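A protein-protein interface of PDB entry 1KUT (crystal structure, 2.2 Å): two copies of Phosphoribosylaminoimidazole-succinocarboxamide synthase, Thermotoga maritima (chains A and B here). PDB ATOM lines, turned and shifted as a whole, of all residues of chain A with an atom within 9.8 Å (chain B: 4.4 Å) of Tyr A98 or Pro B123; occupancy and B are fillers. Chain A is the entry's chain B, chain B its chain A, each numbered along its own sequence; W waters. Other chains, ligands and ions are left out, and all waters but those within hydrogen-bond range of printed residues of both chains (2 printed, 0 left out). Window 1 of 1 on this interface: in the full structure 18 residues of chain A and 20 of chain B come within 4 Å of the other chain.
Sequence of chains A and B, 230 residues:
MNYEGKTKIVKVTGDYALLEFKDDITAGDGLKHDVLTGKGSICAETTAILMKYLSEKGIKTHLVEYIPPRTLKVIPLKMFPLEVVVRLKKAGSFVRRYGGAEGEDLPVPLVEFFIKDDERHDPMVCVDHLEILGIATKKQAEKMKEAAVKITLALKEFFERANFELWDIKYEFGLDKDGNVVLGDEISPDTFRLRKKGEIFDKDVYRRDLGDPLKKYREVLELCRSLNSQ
NH1 of Arg B120 sits at hydrogen-bond distance from O of Val A95 (3.3 Å).
The backbone carbonyl oxygen (O) of Arg A96 lies within hydrogen-bond range of the guanidinium group (NH1) of Arg B120, at 3.1 Å.
OH of Tyr A98 is in hydrogen-bond range of O of Met B124.
A ring nitrogen (NE2) of His B129 lies close to the side-chain carboxylate (OE2) of Glu A112, at 3.5 Å.
The guanidinium group (NE) of Arg B120 sits close to the backbone NH (N) of Gly A99.
Among the printed residues, merely in contact across the chains: Arg A97 with Arg B120 (3.2 Å), Arg A97 with Pro B123 (3.1 Å), Tyr A98 with Ile B115 (3.9 Å), Tyr A98 with Arg B120 (3.9 Å), Tyr A98 with Pro B123 (3.6 Å), Tyr A98 with Val B125 (3.4 Å), Tyr A98 with His B129 (3.8 Å), Tyr A98 with Leu B133 (3.99 Å), Leu A110 with His B129 (3.9 Å), Met A124 with Met B124 (2.9 Å), Met A124 with His B129 (3.98 Å) and Val A125 with Met B124 (3.997 Å).
Of the printed residues of chain B, Arg A97 touches Arg B120 (3.2 Å) and Pro B123 (3.1 Å).
Ala A101 touches none of the printed residues of chain B.
Leu A106 touches none of the printed residues of chain B.
Printed residues of chain B within 4 Å of Met A124: Met B124 and His B129.
Ile B115 touches just one residue of chain A: Tyr A98.
Pro B123 touches two residues of chain A.
The nearest printed residue of chain B that does not touch Tyr A98 is Asp B122 (6.8 Å).
Met B124 touches its own counterpart, Met A124.
Val A125 touches Met B124, but with the chains exchanged Met A124 does not touch Val B125 (4.2 Å).
4 positions are printed for both chains.
O of Phe B113 lies within hydrogen-bond range of N of Val B125, at 3.1 Å.
N of Ile B115 is in hydrogen-bond range of O of Pro B123 (3.1 Å).
NE of Arg A87 lies within salt-bridge range of OE1 of Glu A112, 2.6 Å away.
The backbone carbonyl oxygen (O) of Ser A93 is in hydrogen-bond range of the guanidinium group (NE) of Arg A97 (2.7 Å).
The guanidinium group (NH1) of Arg A97 lies within hydrogen-bond range of the side-chain sulfur (SD) of Met A124, at 3.5 Å.
N of Val A125 sits at hydrogen-bond distance from O of Phe A113 (2.9 Å).
Of the 11 printed residues of chain B, 7 touch a printed residue of chain A.
Printed residues of chain B that touch a printed residue of chain A: Ile B115, Arg B120, Pro B123, Met B124, Val B125, His B129 and Leu B133.
Hydrophobic or aromatic side chains of chain B that line the printed part of chain A: Ile B115, Pro B123, Met B124, Val B125, His B129 and Leu B133.
Of the 24 printed residues of chain A, 9 touch a printed residue of chain B.
Hydrophobic or aromatic side chains of chain A within 4 Å of the printed part of chain B: Tyr A98, Leu A110 and Met A124.
Among the printed residues, no Asp or Glu carboxylate lies within 4 Å of a Lys or Arg side-chain nitrogen of the other chain.
Water W1 lies within hydrogen-bond range of O of Val B125 (2.8 Å), N of Phe B113 (2.8 Å) and SG of Cys A126 (3.5 Å).
Water W2 lies within hydrogen-bond range of the guanidinium group of Arg B120 and the backbone NH of Gly A100.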
ATOM      1  N   ARG A  87     -10.900 -18.204  -6.746  1.00  0.00           N
ATOM      2  CA  ARG A  87      -9.823 -18.248  -7.714  1.00  0.00           C
ATOM      3  C   ARG A  87      -8.595 -18.871  -7.088  1.00  0.00           C
ATOM      4  O   ARG A  87      -8.227 -18.538  -5.964  1.00  0.00           O
ATOM      5  CB  ARG A  87      -9.487 -16.841  -8.209  1.00  0.00           C
ATOM      6  CG  ARG A  87     -10.638 -16.167  -8.935  1.00  0.00           C
ATOM      7  CD  ARG A  87     -10.337 -14.721  -9.213  1.00  0.00           C
ATOM      8  NE  ARG A  87     -11.542 -14.020  -9.641  1.00  0.00           N
ATOM      9  CZ  ARG A  87     -12.118 -14.163 -10.831  1.00  0.00           C
ATOM     10  NH1 ARG A  87     -11.593 -14.982 -11.730  1.00  0.00           N
ATOM     11  NH2 ARG A  87     -13.227 -13.489 -11.112  1.00  0.00           N
ATOM     12  N   LYS A  90      -4.723 -16.900 -11.513  1.00  0.00           N
ATOM     13  CA  LYS A  90      -5.136 -15.660 -12.158  1.00  0.00           C
ATOM     14  C   LYS A  90      -5.692 -15.926 -13.544  1.00  0.00           C
ATOM     15  O   LYS A  90      -4.990 -16.448 -14.405  1.00  0.00           O
ATOM     16  CB  LYS A  90      -3.950 -14.698 -12.284  1.00  0.00           C
ATOM     17  CG  LYS A  90      -3.286 -14.295 -10.982  1.00  0.00           C
ATOM     18  CD  LYS A  90      -2.110 -13.363 -11.277  1.00  0.00           C
ATOM     19  CE  LYS A  90      -1.315 -13.001 -10.023  1.00  0.00           C
ATOM     20  NZ  LYS A  90      -0.019 -12.315 -10.367  1.00  0.00           N
ATOM     21  N   ALA A  91      -6.943 -15.541 -13.770  1.00  0.00           N
ATOM     22  CA  ALA A  91      -7.564 -15.744 -15.067  1.00  0.00           C
ATOM     23  C   ALA A  91      -8.829 -14.918 -15.246  1.00  0.00           C
ATOM     24  O   ALA A  91      -9.422 -14.442 -14.274  1.00  0.00           O
ATOM     25  CB  ALA A  91      -7.880 -17.200 -15.246  1.00  0.00           C
ATOM     26  N   GLY A  92      -9.232 -14.741 -16.502  1.00  0.00           N
ATOM     27  CA  GLY A  92     -10.445 -13.997 -16.810  1.00  0.00           C
ATOM     28  C   GLY A  92     -10.547 -12.534 -16.401  1.00  0.00           C
ATOM     29  O   GLY A  92      -9.654 -11.726 -16.676  1.00  0.00           O
ATOM     30  N   SER A  93     -11.660 -12.194 -15.756  1.00  0.00           N
ATOM     31  CA  SER A  93     -11.912 -10.836 -15.314  1.00  0.00           C
ATOM     32  C   SER A  93     -10.897 -10.439 -14.253  1.00  0.00           C
ATOM     33  O   SER A  93     -10.764  -9.252 -13.919  1.00  0.00           O
ATOM     34  CB  SER A  93     -13.309 -10.735 -14.721  1.00  0.00           C
ATOM     35  OG  SER A  93     -13.365 -11.423 -13.480  1.00  0.00           O
ATOM     36  N   PHE A  94     -10.182 -11.423 -13.714  1.00  0.00           N
ATOM     37  CA  PHE A  94      -9.200 -11.103 -12.693  1.00  0.00           C
ATOM     38  C   PHE A  94      -7.975 -10.455 -13.307  1.00  0.00           C
ATOM     39  O   PHE A  94      -7.406  -9.541 -12.724  1.00  0.00           O
ATOM     40  CB  PHE A  94      -8.768 -12.338 -11.903  1.00  0.00           C
ATOM     41  CG  PHE A  94      -7.867 -12.012 -10.729  1.00  0.00           C
ATOM     42  CD1 PHE A  94      -8.409 -11.676  -9.491  1.00  0.00           C
ATOM     43  CD2 PHE A  94      -6.478 -11.989 -10.883  1.00  0.00           C
ATOM     44  CE1 PHE A  94      -7.582 -11.322  -8.430  1.00  0.00           C
ATOM     45  CE2 PHE A  94      -5.643 -11.635  -9.829  1.00  0.00           C
ATOM     46  CZ  PHE A  94      -6.190 -11.302  -8.602  1.00  0.00           C
ATOM     47  N   VAL A  95      -7.548 -10.929 -14.471  1.00  0.00           N
ATOM     48  CA  VAL A  95      -6.385 -10.328 -15.108  1.00  0.00           C
ATOM     49  C   VAL A  95      -6.767  -8.990 -15.737  1.00  0.00           C
ATOM     50  O   VAL A  95      -5.974  -8.050 -15.764  1.00  0.00           O
ATOM     51  CB  VAL A  95      -5.769 -11.266 -16.167  1.00  0.00           C
ATOM     52  CG1 VAL A  95      -5.064 -12.428 -15.471  1.00  0.00           C
ATOM     53  CG2 VAL A  95      -6.853 -11.800 -17.100  1.00  0.00           C
ATOM     54  N   ARG A  96      -8.005  -8.889 -16.208  1.00  0.00           N
ATOM     55  CA  ARG A  96      -8.461  -7.648 -16.815  1.00  0.00           C
ATOM     56  C   ARG A  96      -8.668  -6.524 -15.795  1.00  0.00           C
ATOM     57  O   ARG A  96      -8.724  -5.351 -16.160  1.00  0.00           O
ATOM     58  CB  ARG A  96      -9.759  -7.892 -17.591  1.00  0.00           C
ATOM     59  CG  ARG A  96      -9.617  -8.952 -18.690  1.00  0.00           C
ATOM     60  CD  ARG A  96     -10.735  -8.838 -19.706  1.00  0.00           C
ATOM     61  NE  ARG A  96     -12.048  -9.093 -19.123  1.00  0.00           N
ATOM     62  CZ  ARG A  96     -12.542 -10.302 -18.860  1.00  0.00           C
ATOM     63  NH1 ARG A  96     -11.836 -11.398 -19.131  1.00  0.00           N
ATOM     64  NH2 ARG A  96     -13.750 -10.412 -18.316  1.00  0.00           N
ATOM     65  N   ARG A  97      -8.773  -6.870 -14.519  1.00  0.00           N
ATOM     66  CA  ARG A  97      -8.978  -5.852 -13.487  1.00  0.00           C
ATOM     67  C   ARG A  97      -7.709  -5.497 -12.720  1.00  0.00           C
ATOM     68  O   ARG A  97      -7.483  -4.338 -12.378  1.00  0.00           O
ATOM     69  CB  ARG A  97     -10.023  -6.322 -12.468  1.00  0.00           C
ATOM     70  CG  ARG A  97     -11.462  -6.285 -12.926  1.00  0.00           C
ATOM     71  CD  ARG A  97     -12.352  -6.885 -11.851  1.00  0.00           C
ATOM     72  NE  ARG A  97     -12.236  -8.340 -11.842  1.00  0.00           N
ATOM     73  CZ  ARG A  97     -12.363  -9.099 -10.758  1.00  0.00           C
ATOM     74  NH1 ARG A  97     -12.607  -8.539  -9.573  1.00  0.00           N
ATOM     75  NH2 ARG A  97     -12.263 -10.419 -10.865  1.00  0.00           N
ATOM     76  N   TYR A  98      -6.879  -6.503 -12.466  1.00  0.00           N
ATOM     77  CA  TYR A  98      -5.676  -6.305 -11.677  1.00  0.00           C
ATOM     78  C   TYR A  98      -4.375  -6.660 -12.378  1.00  0.00           C
ATOM     79  O   TYR A  98      -3.305  -6.585 -11.767  1.00  0.00           O
ATOM     80  CB  TYR A  98      -5.801  -7.141 -10.406  1.00  0.00           C
ATOM     81  CG  TYR A  98      -7.142  -6.984  -9.737  1.00  0.00           C
ATOM     82  CD1 TYR A  98      -7.587  -5.727  -9.334  1.00  0.00           C
ATOM     83  CD2 TYR A  98      -7.979  -8.081  -9.529  1.00  0.00           C
ATOM     84  CE1 TYR A  98      -8.836  -5.555  -8.739  1.00  0.00           C
ATOM     85  CE2 TYR A  98      -9.242  -7.925  -8.928  1.00  0.00           C
ATOM     86  CZ  TYR A  98      -9.663  -6.658  -8.536  1.00  0.00           C
ATOM     87  OH  TYR A  98     -10.894  -6.475  -7.927  1.00  0.00           O
ATOM     88  N   GLY A  99      -4.455  -7.057 -13.644  1.00  0.00           N
ATOM     89  CA  GLY A  99      -3.247  -7.434 -14.359  1.00  0.00           C
ATOM     90  C   GLY A  99      -2.706  -8.774 -13.869  1.00  0.00           C
ATOM     91  O   GLY A  99      -3.404  -9.535 -13.189  1.00  0.00           O
ATOM     92  N   GLY A 100      -1.457  -9.071 -14.211  1.00  0.00           N
ATOM     93  CA  GLY A 100      -0.863 -10.325 -13.784  1.00  0.00           C
ATOM     94  C   GLY A 100      -0.706 -11.303 -14.930  1.00  0.00           C
ATOM     95  O   GLY A 100      -1.040 -10.987 -16.078  1.00  0.00           O
ATOM     96  N   ALA A 101      -0.199 -12.495 -14.626  1.00  0.00           N
ATOM     97  CA  ALA A 101       0.008 -13.509 -15.653  1.00  0.00           C
ATOM     98  C   ALA A 101      -1.117 -14.516 -15.643  1.00  0.00           C
ATOM     99  O   ALA A 101      -1.235 -15.285 -14.695  1.00  0.00           O
ATOM    100  CB  ALA A 101       1.328 -14.221 -15.421  1.00  0.00           C
ATOM    101  N   GLU A 102      -1.947 -14.517 -16.683  1.00  0.00           N
ATOM    102  CA  GLU A 102      -3.044 -15.480 -16.745  1.00  0.00           C
ATOM    103  C   GLU A 102      -2.477 -16.890 -16.624  1.00  0.00           C
ATOM    104  O   GLU A 102      -1.694 -17.335 -17.467  1.00  0.00           O
ATOM    105  CB  GLU A 102      -3.816 -15.366 -18.058  1.00  0.00           C
ATOM    106  CG  GLU A 102      -5.013 -16.305 -18.130  1.00  0.00           C
ATOM    107  CD  GLU A 102      -5.807 -16.147 -19.409  1.00  0.00           C
ATOM    108  OE1 GLU A 102      -5.301 -16.562 -20.478  1.00  0.00           O
ATOM    109  OE2 GLU A 102      -6.936 -15.601 -19.348  1.00  0.00           O
ATOM    110  N   GLU A 104      -1.076 -17.735 -13.688  1.00  0.00           N
ATOM    111  CA  GLU A 104      -0.217 -17.640 -12.517  1.00  0.00           C
ATOM    112  C   GLU A 104      -1.020 -18.041 -11.302  1.00  0.00           C
ATOM    113  O   GLU A 104      -2.213 -17.740 -11.194  1.00  0.00           O
ATOM    114  CB  GLU A 104       0.340 -16.222 -12.293  1.00  0.00           C
ATOM    115  CG  GLU A 104       1.370 -16.194 -11.130  1.00  0.00           C
ATOM    116  CD  GLU A 104       1.913 -14.804 -10.783  1.00  0.00           C
ATOM    117  OE1 GLU A 104       2.505 -14.153 -11.671  1.00  0.00           O
ATOM    118  OE2 GLU A 104       1.752 -14.368  -9.615  1.00  0.00           O
ATOM    119  N   LEU A 106      -2.110 -18.123  -7.323  1.00  0.00           N
ATOM    120  CA  LEU A 106      -2.367 -17.084  -6.353  1.00  0.00           C
ATOM    121  C   LEU A 106      -1.642 -17.658  -5.157  1.00  0.00           C
ATOM    122  O   LEU A 106      -1.369 -18.855  -5.133  1.00  0.00           O
ATOM    123  CB  LEU A 106      -3.870 -16.957  -6.081  1.00  0.00           C
ATOM    124  CG  LEU A 106      -4.663 -16.370  -7.254  1.00  0.00           C
ATOM    125  CD1 LEU A 106      -6.142 -16.320  -6.913  1.00  0.00           C
ATOM    126  CD2 LEU A 106      -4.128 -14.964  -7.578  1.00  0.00           C
ATOM    127  N   LEU A 110      -8.631 -17.072  -3.542  1.00  0.00           N
ATOM    128  CA  LEU A 110      -9.363 -15.818  -3.462  1.00  0.00           C
ATOM    129  C   LEU A 110     -10.861 -16.022  -3.709  1.00  0.00           C
ATOM    130  O   LEU A 110     -11.261 -16.642  -4.708  1.00  0.00           O
ATOM    131  CB  LEU A 110      -8.796 -14.833  -4.475  1.00  0.00           C
ATOM    132  CG  LEU A 110      -9.527 -13.501  -4.591  1.00  0.00           C
ATOM    133  CD1 LEU A 110      -9.368 -12.677  -3.316  1.00  0.00           C
ATOM    134  CD2 LEU A 110      -8.981 -12.775  -5.782  1.00  0.00           C
ATOM    135  N   VAL A 111     -11.674 -15.515  -2.780  1.00  0.00           N
ATOM    136  CA  VAL A 111     -13.128 -15.596  -2.864  1.00  0.00           C
ATOM    137  C   VAL A 111     -13.701 -14.221  -3.190  1.00  0.00           C
ATOM    138  O   VAL A 111     -13.403 -13.261  -2.491  1.00  0.00           O
ATOM    139  CB  VAL A 111     -13.755 -16.023  -1.528  1.00  0.00           C
ATOM    140  CG1 VAL A 111     -15.235 -16.293  -1.727  1.00  0.00           C
ATOM    141  CG2 VAL A 111     -13.045 -17.241  -0.979  1.00  0.00           C
ATOM    142  N   GLU A 112     -14.533 -14.142  -4.233  1.00  0.00           N
ATOM    143  CA  GLU A 112     -15.171 -12.899  -4.670  1.00  0.00           C
ATOM    144  C   GLU A 112     -16.688 -13.060  -4.767  1.00  0.00           C
ATOM    145  O   GLU A 112     -17.181 -14.090  -5.237  1.00  0.00           O
ATOM    146  CB  GLU A 112     -14.695 -12.498  -6.070  1.00  0.00           C
ATOM    147  CG  GLU A 112     -13.246 -12.090  -6.213  1.00  0.00           C
ATOM    148  CD  GLU A 112     -12.964 -11.438  -7.574  1.00  0.00           C
ATOM    149  OE1 GLU A 112     -12.983 -12.135  -8.620  1.00  0.00           O
ATOM    150  OE2 GLU A 112     -12.734 -10.214  -7.594  1.00  0.00           O
ATOM    151  N   PHE A 113     -17.434 -12.039  -4.358  1.00  0.00           N
ATOM    152  CA  PHE A 113     -18.885 -12.102  -4.479  1.00  0.00           C
ATOM    153  C   PHE A 113     -19.370 -11.185  -5.595  1.00  0.00           C
ATOM    154  O   PHE A 113     -18.844 -10.097  -5.814  1.00  0.00           O
ATOM    155  CB  PHE A 113     -19.585 -11.704  -3.181  1.00  0.00           C
ATOM    156  CG  PHE A 113     -19.449 -12.708  -2.079  1.00  0.00           C
ATOM    157  CD1 PHE A 113     -18.290 -12.763  -1.305  1.00  0.00           C
ATOM    158  CD2 PHE A 113     -20.489 -13.602  -1.802  1.00  0.00           C
ATOM    159  CE1 PHE A 113     -18.171 -13.693  -0.267  1.00  0.00           C
ATOM    160  CE2 PHE A 113     -20.374 -14.535  -0.763  1.00  0.00           C
ATOM    161  CZ  PHE A 113     -19.214 -14.582   0.005  1.00  0.00           C
ATOM    162  N   PHE A 114     -20.394 -11.640  -6.294  1.00  0.00           N
ATOM    163  CA  PHE A 114     -20.999 -10.886  -7.377  1.00  0.00           C
ATOM    164  C   PHE A 114     -22.509 -10.977  -7.240  1.00  0.00           C
ATOM    165  O   PHE A 114     -23.074 -12.065  -7.106  1.00  0.00           O
ATOM    166  CB  PHE A 114     -20.606 -11.478  -8.724  1.00  0.00           C
ATOM    167  CG  PHE A 114     -19.179 -11.259  -9.082  1.00  0.00           C
ATOM    168  CD1 PHE A 114     -18.795 -10.121  -9.788  1.00  0.00           C
ATOM    169  CD2 PHE A 114     -18.207 -12.198  -8.726  1.00  0.00           C
ATOM    170  CE1 PHE A 114     -17.462  -9.919 -10.143  1.00  0.00           C
ATOM    171  CE2 PHE A 114     -16.865 -12.006  -9.073  1.00  0.00           C
ATOM    172  CZ  PHE A 114     -16.491 -10.865  -9.787  1.00  0.00           C
ATOM    173  N   MET A 124     -19.583  -6.729  -8.513  1.00  0.00           N
ATOM    174  CA  MET A 124     -18.909  -7.349  -7.396  1.00  0.00           C
ATOM    175  C   MET A 124     -19.357  -6.669  -6.115  1.00  0.00           C
ATOM    176  O   MET A 124     -19.812  -5.537  -6.138  1.00  0.00           O
ATOM    177  CB  MET A 124     -17.391  -7.210  -7.558  1.00  0.00           C
ATOM    178  CG  MET A 124     -16.583  -7.924  -6.466  1.00  0.00           C
ATOM    179  SD  MET A 124     -14.684  -8.028  -6.858  1.00  0.00           S
ATOM    180  CE  MET A 124     -14.228  -6.189  -6.576  1.00  0.00           C
ATOM    181  N   VAL A 125     -19.232  -7.364  -4.995  1.00  0.00           N
ATOM    182  CA  VAL A 125     -19.610  -6.800  -3.704  1.00  0.00           C
ATOM    183  C   VAL A 125     -18.685  -7.367  -2.648  1.00  0.00           C
ATOM    184  O   VAL A 125     -18.056  -8.400  -2.859  1.00  0.00           O
ATOM    185  CB  VAL A 125     -21.075  -7.166  -3.299  1.00  0.00           C
ATOM    186  CG1 VAL A 125     -22.072  -6.271  -4.012  1.00  0.00           C
ATOM    187  CG2 VAL A 125     -21.365  -8.617  -3.634  1.00  0.00           C
ATOM    188  N   CYS A 126     -18.593  -6.674  -1.519  1.00  0.00           N
ATOM    189  CA  CYS A 126     -17.787  -7.116  -0.388  1.00  0.00           C
ATOM    190  C   CYS A 126     -18.851  -7.408   0.675  1.00  0.00           C
ATOM    191  O   CYS A 126     -20.014  -7.013   0.504  1.00  0.00           O
ATOM    192  CB  CYS A 126     -16.825  -6.010   0.064  1.00  0.00           C
ATOM    193  SG  CYS A 126     -15.647  -5.470  -1.233  1.00  0.00           S
ATOM    194  N   PHE B 113     -13.248   0.389  -1.460  1.00  0.00           N
ATOM    195  CA  PHE B 113     -11.880   0.650  -1.881  1.00  0.00           C
ATOM    196  C   PHE B 113     -11.746   0.538  -3.387  1.00  0.00           C
ATOM    197  O   PHE B 113     -12.317  -0.345  -4.005  1.00  0.00           O
ATOM    198  CB  PHE B 113     -10.891  -0.349  -1.243  1.00  0.00           C
ATOM    199  CG  PHE B 113     -10.645  -0.124   0.224  1.00  0.00           C
ATOM    200  CD1 PHE B 113     -11.507  -0.629   1.177  1.00  0.00           C
ATOM    201  CD2 PHE B 113      -9.545   0.612   0.651  1.00  0.00           C
ATOM    202  CE1 PHE B 113     -11.273  -0.403   2.548  1.00  0.00           C
ATOM    203  CE2 PHE B 113      -9.311   0.836   2.007  1.00  0.00           C
ATOM    204  CZ  PHE B 113     -10.171   0.330   2.952  1.00  0.00           C
ATOM    205  N   PHE B 114     -10.954   1.423  -3.970  1.00  0.00           N
ATOM    206  CA  PHE B 114     -10.717   1.406  -5.409  1.00  0.00           C
ATOM    207  C   PHE B 114      -9.230   1.601  -5.669  1.00  0.00           C
ATOM    208  O   PHE B 114      -8.589   2.479  -5.084  1.00  0.00           O
ATOM    209  CB  PHE B 114     -11.498   2.532  -6.099  1.00  0.00           C
ATOM    210  CG  PHE B 114     -12.988   2.376  -6.004  1.00  0.00           C
ATOM    211  CD1 PHE B 114     -13.644   1.427  -6.762  1.00  0.00           C
ATOM    212  CD2 PHE B 114     -13.718   3.148  -5.127  1.00  0.00           C
ATOM    213  CE1 PHE B 114     -15.018   1.237  -6.647  1.00  0.00           C
ATOM    214  CE2 PHE B 114     -15.096   2.968  -5.001  1.00  0.00           C
ATOM    215  CZ  PHE B 114     -15.743   2.002  -5.768  1.00  0.00           C
ATOM    216  N   ILE B 115      -8.681   0.752  -6.523  1.00  0.00           N
ATOM    217  CA  ILE B 115      -7.282   0.849  -6.895  1.00  0.00           C
ATOM    218  C   ILE B 115      -7.181   1.999  -7.884  1.00  0.00           C
ATOM    219  O   ILE B 115      -8.094   2.221  -8.686  1.00  0.00           O
ATOM    220  CB  ILE B 115      -6.804  -0.447  -7.582  1.00  0.00           C
ATOM    221  CG1 ILE B 115      -6.589  -1.535  -6.534  1.00  0.00           C
ATOM    222  CG2 ILE B 115      -5.535  -0.191  -8.371  1.00  0.00           C
ATOM    223  CD1 ILE B 115      -6.174  -2.865  -7.125  1.00  0.00           C
ATOM    224  N   ARG B 120      -7.006   0.420 -16.149  1.00  0.00           N
ATOM    225  CA  ARG B 120      -7.877  -0.689 -15.772  1.00  0.00           C
ATOM    226  C   ARG B 120      -9.183  -0.233 -15.133  1.00  0.00           C
ATOM    227  O   ARG B 120      -9.922  -1.030 -14.556  1.00  0.00           O
ATOM    228  CB  ARG B 120      -7.134  -1.656 -14.850  1.00  0.00           C
ATOM    229  CG  ARG B 120      -6.032  -2.402 -15.577  1.00  0.00           C
ATOM    230  CD  ARG B 120      -5.432  -3.494 -14.729  1.00  0.00           C
ATOM    231  NE  ARG B 120      -4.363  -4.205 -15.429  1.00  0.00           N
ATOM    232  CZ  ARG B 120      -4.532  -4.937 -16.529  1.00  0.00           C
ATOM    233  NH1 ARG B 120      -5.734  -5.063 -17.080  1.00  0.00           N
ATOM    234  NH2 ARG B 120      -3.501  -5.571 -17.068  1.00  0.00           N
ATOM    235  N   HIS B 121      -9.445   1.063 -15.227  1.00  0.00           N
ATOM    236  CA  HIS B 121     -10.675   1.646 -14.718  1.00  0.00           C
ATOM    237  C   HIS B 121     -10.915   1.568 -13.218  1.00  0.00           C
ATOM    238  O   HIS B 121     -12.048   1.378 -12.772  1.00  0.00           O
ATOM    239  CB  HIS B 121     -11.838   1.035 -15.488  1.00  0.00           C
ATOM    240  CG  HIS B 121     -11.651   1.112 -16.970  1.00  0.00           C
ATOM    241  ND1 HIS B 121     -11.997   0.086 -17.824  1.00  0.00           N
ATOM    242  CD2 HIS B 121     -11.076   2.067 -17.739  1.00  0.00           C
ATOM    243  CE1 HIS B 121     -11.635   0.404 -19.054  1.00  0.00           C
ATOM    244  NE2 HIS B 121     -11.073   1.600 -19.029  1.00  0.00           N
ATOM    245  N   ASP B 122      -9.843   1.743 -12.452  1.00  0.00           N
ATOM    246  CA  ASP B 122      -9.903   1.740 -10.988  1.00  0.00           C
ATOM    247  C   ASP B 122     -10.845   0.686 -10.416  1.00  0.00           C
ATOM    248  O   ASP B 122     -11.857   1.023  -9.809  1.00  0.00           O
ATOM    249  CB  ASP B 122     -10.335   3.124 -10.466  1.00  0.00           C
ATOM    250  CG  ASP B 122      -9.597   4.280 -11.151  1.00  0.00           C
ATOM    251  OD1 ASP B 122      -8.345   4.227 -11.276  1.00  0.00           O
ATOM    252  OD2 ASP B 122     -10.276   5.254 -11.553  1.00  0.00           O
ATOM    253  N   PRO B 123     -10.513  -0.604 -10.592  1.00  0.00           N
ATOM    254  CA  PRO B 123     -11.354  -1.686 -10.078  1.00  0.00           C
ATOM    255  C   PRO B 123     -11.504  -1.674  -8.552  1.00  0.00           C
ATOM    256  O   PRO B 123     -10.572  -1.338  -7.814  1.00  0.00           O
ATOM    257  CB  PRO B 123     -10.636  -2.944 -10.579  1.00  0.00           C
ATOM    258  CG  PRO B 123      -9.196  -2.533 -10.599  1.00  0.00           C
ATOM    259  CD  PRO B 123      -9.276  -1.141 -11.195  1.00  0.00           C
ATOM    260  N   MET B 124     -12.691  -2.025  -8.082  1.00  0.00           N
ATOM    261  CA  MET B 124     -12.933  -2.088  -6.652  1.00  0.00           C
ATOM    262  C   MET B 124     -12.222  -3.324  -6.097  1.00  0.00           C
ATOM    263  O   MET B 124     -11.988  -4.306  -6.815  1.00  0.00           O
ATOM    264  CB  MET B 124     -14.441  -2.170  -6.373  1.00  0.00           C
ATOM    265  CG  MET B 124     -14.776  -2.354  -4.913  1.00  0.00           C
ATOM    266  SD  MET B 124     -16.659  -2.149  -4.589  1.00  0.00           S
ATOM    267  CE  MET B 124     -17.230  -3.908  -5.151  1.00  0.00           C
ATOM    268  N   VAL B 125     -11.848  -3.268  -4.825  1.00  0.00           N
ATOM    269  CA  VAL B 125     -11.183  -4.398  -4.185  1.00  0.00           C
ATOM    270  C   VAL B 125     -11.624  -4.537  -2.732  1.00  0.00           C
ATOM    271  O   VAL B 125     -11.713  -3.540  -2.005  1.00  0.00           O
ATOM    272  CB  VAL B 125      -9.651  -4.229  -4.173  1.00  0.00           C
ATOM    273  CG1 VAL B 125      -9.069  -4.449  -5.543  1.00  0.00           C
ATOM    274  CG2 VAL B 125      -9.301  -2.823  -3.654  1.00  0.00           C
ATOM    275  N   HIS B 129      -8.449  -8.756  -1.241  1.00  0.00           N
ATOM    276  CA  HIS B 129      -7.761  -8.358  -2.458  1.00  0.00           C
ATOM    277  C   HIS B 129      -6.533  -7.524  -2.108  1.00  0.00           C
ATOM    278  O   HIS B 129      -5.424  -7.807  -2.572  1.00  0.00           O
ATOM    279  CB  HIS B 129      -8.676  -7.496  -3.323  1.00  0.00           C
ATOM    280  CG  HIS B 129      -9.817  -8.238  -3.933  1.00  0.00           C
ATOM    281  ND1 HIS B 129      -9.732  -8.842  -5.168  1.00  0.00           N
ATOM    282  CD2 HIS B 129     -11.076  -8.455  -3.488  1.00  0.00           C
ATOM    283  CE1 HIS B 129     -10.894  -9.398  -5.460  1.00  0.00           C
ATOM    284  NE2 HIS B 129     -11.725  -9.176  -4.459  1.00  0.00           N
ATOM    285  N   LEU B 133      -3.101  -8.862  -3.159  1.00  0.00           N
ATOM    286  CA  LEU B 133      -2.441  -8.081  -4.198  1.00  0.00           C
ATOM    287  C   LEU B 133      -1.177  -7.371  -3.716  1.00  0.00           C
ATOM    288  O   LEU B 133      -0.497  -6.729  -4.504  1.00  0.00           O
ATOM    289  CB  LEU B 133      -3.414  -7.061  -4.784  1.00  0.00           C
ATOM    290  CG  LEU B 133      -4.466  -7.639  -5.735  1.00  0.00           C
ATOM    291  CD1 LEU B 133      -5.559  -6.615  -5.957  1.00  0.00           C
ATOM    292  CD2 LEU B 133      -3.815  -8.033  -7.068  1.00  0.00           C
HETATM  293  O   HOH W   1     -14.050  -2.301  -1.212  1.00  0.00           O
HETATM  294  O   HOH W   2      -0.827  -7.092 -16.988  1.00  0.00           O
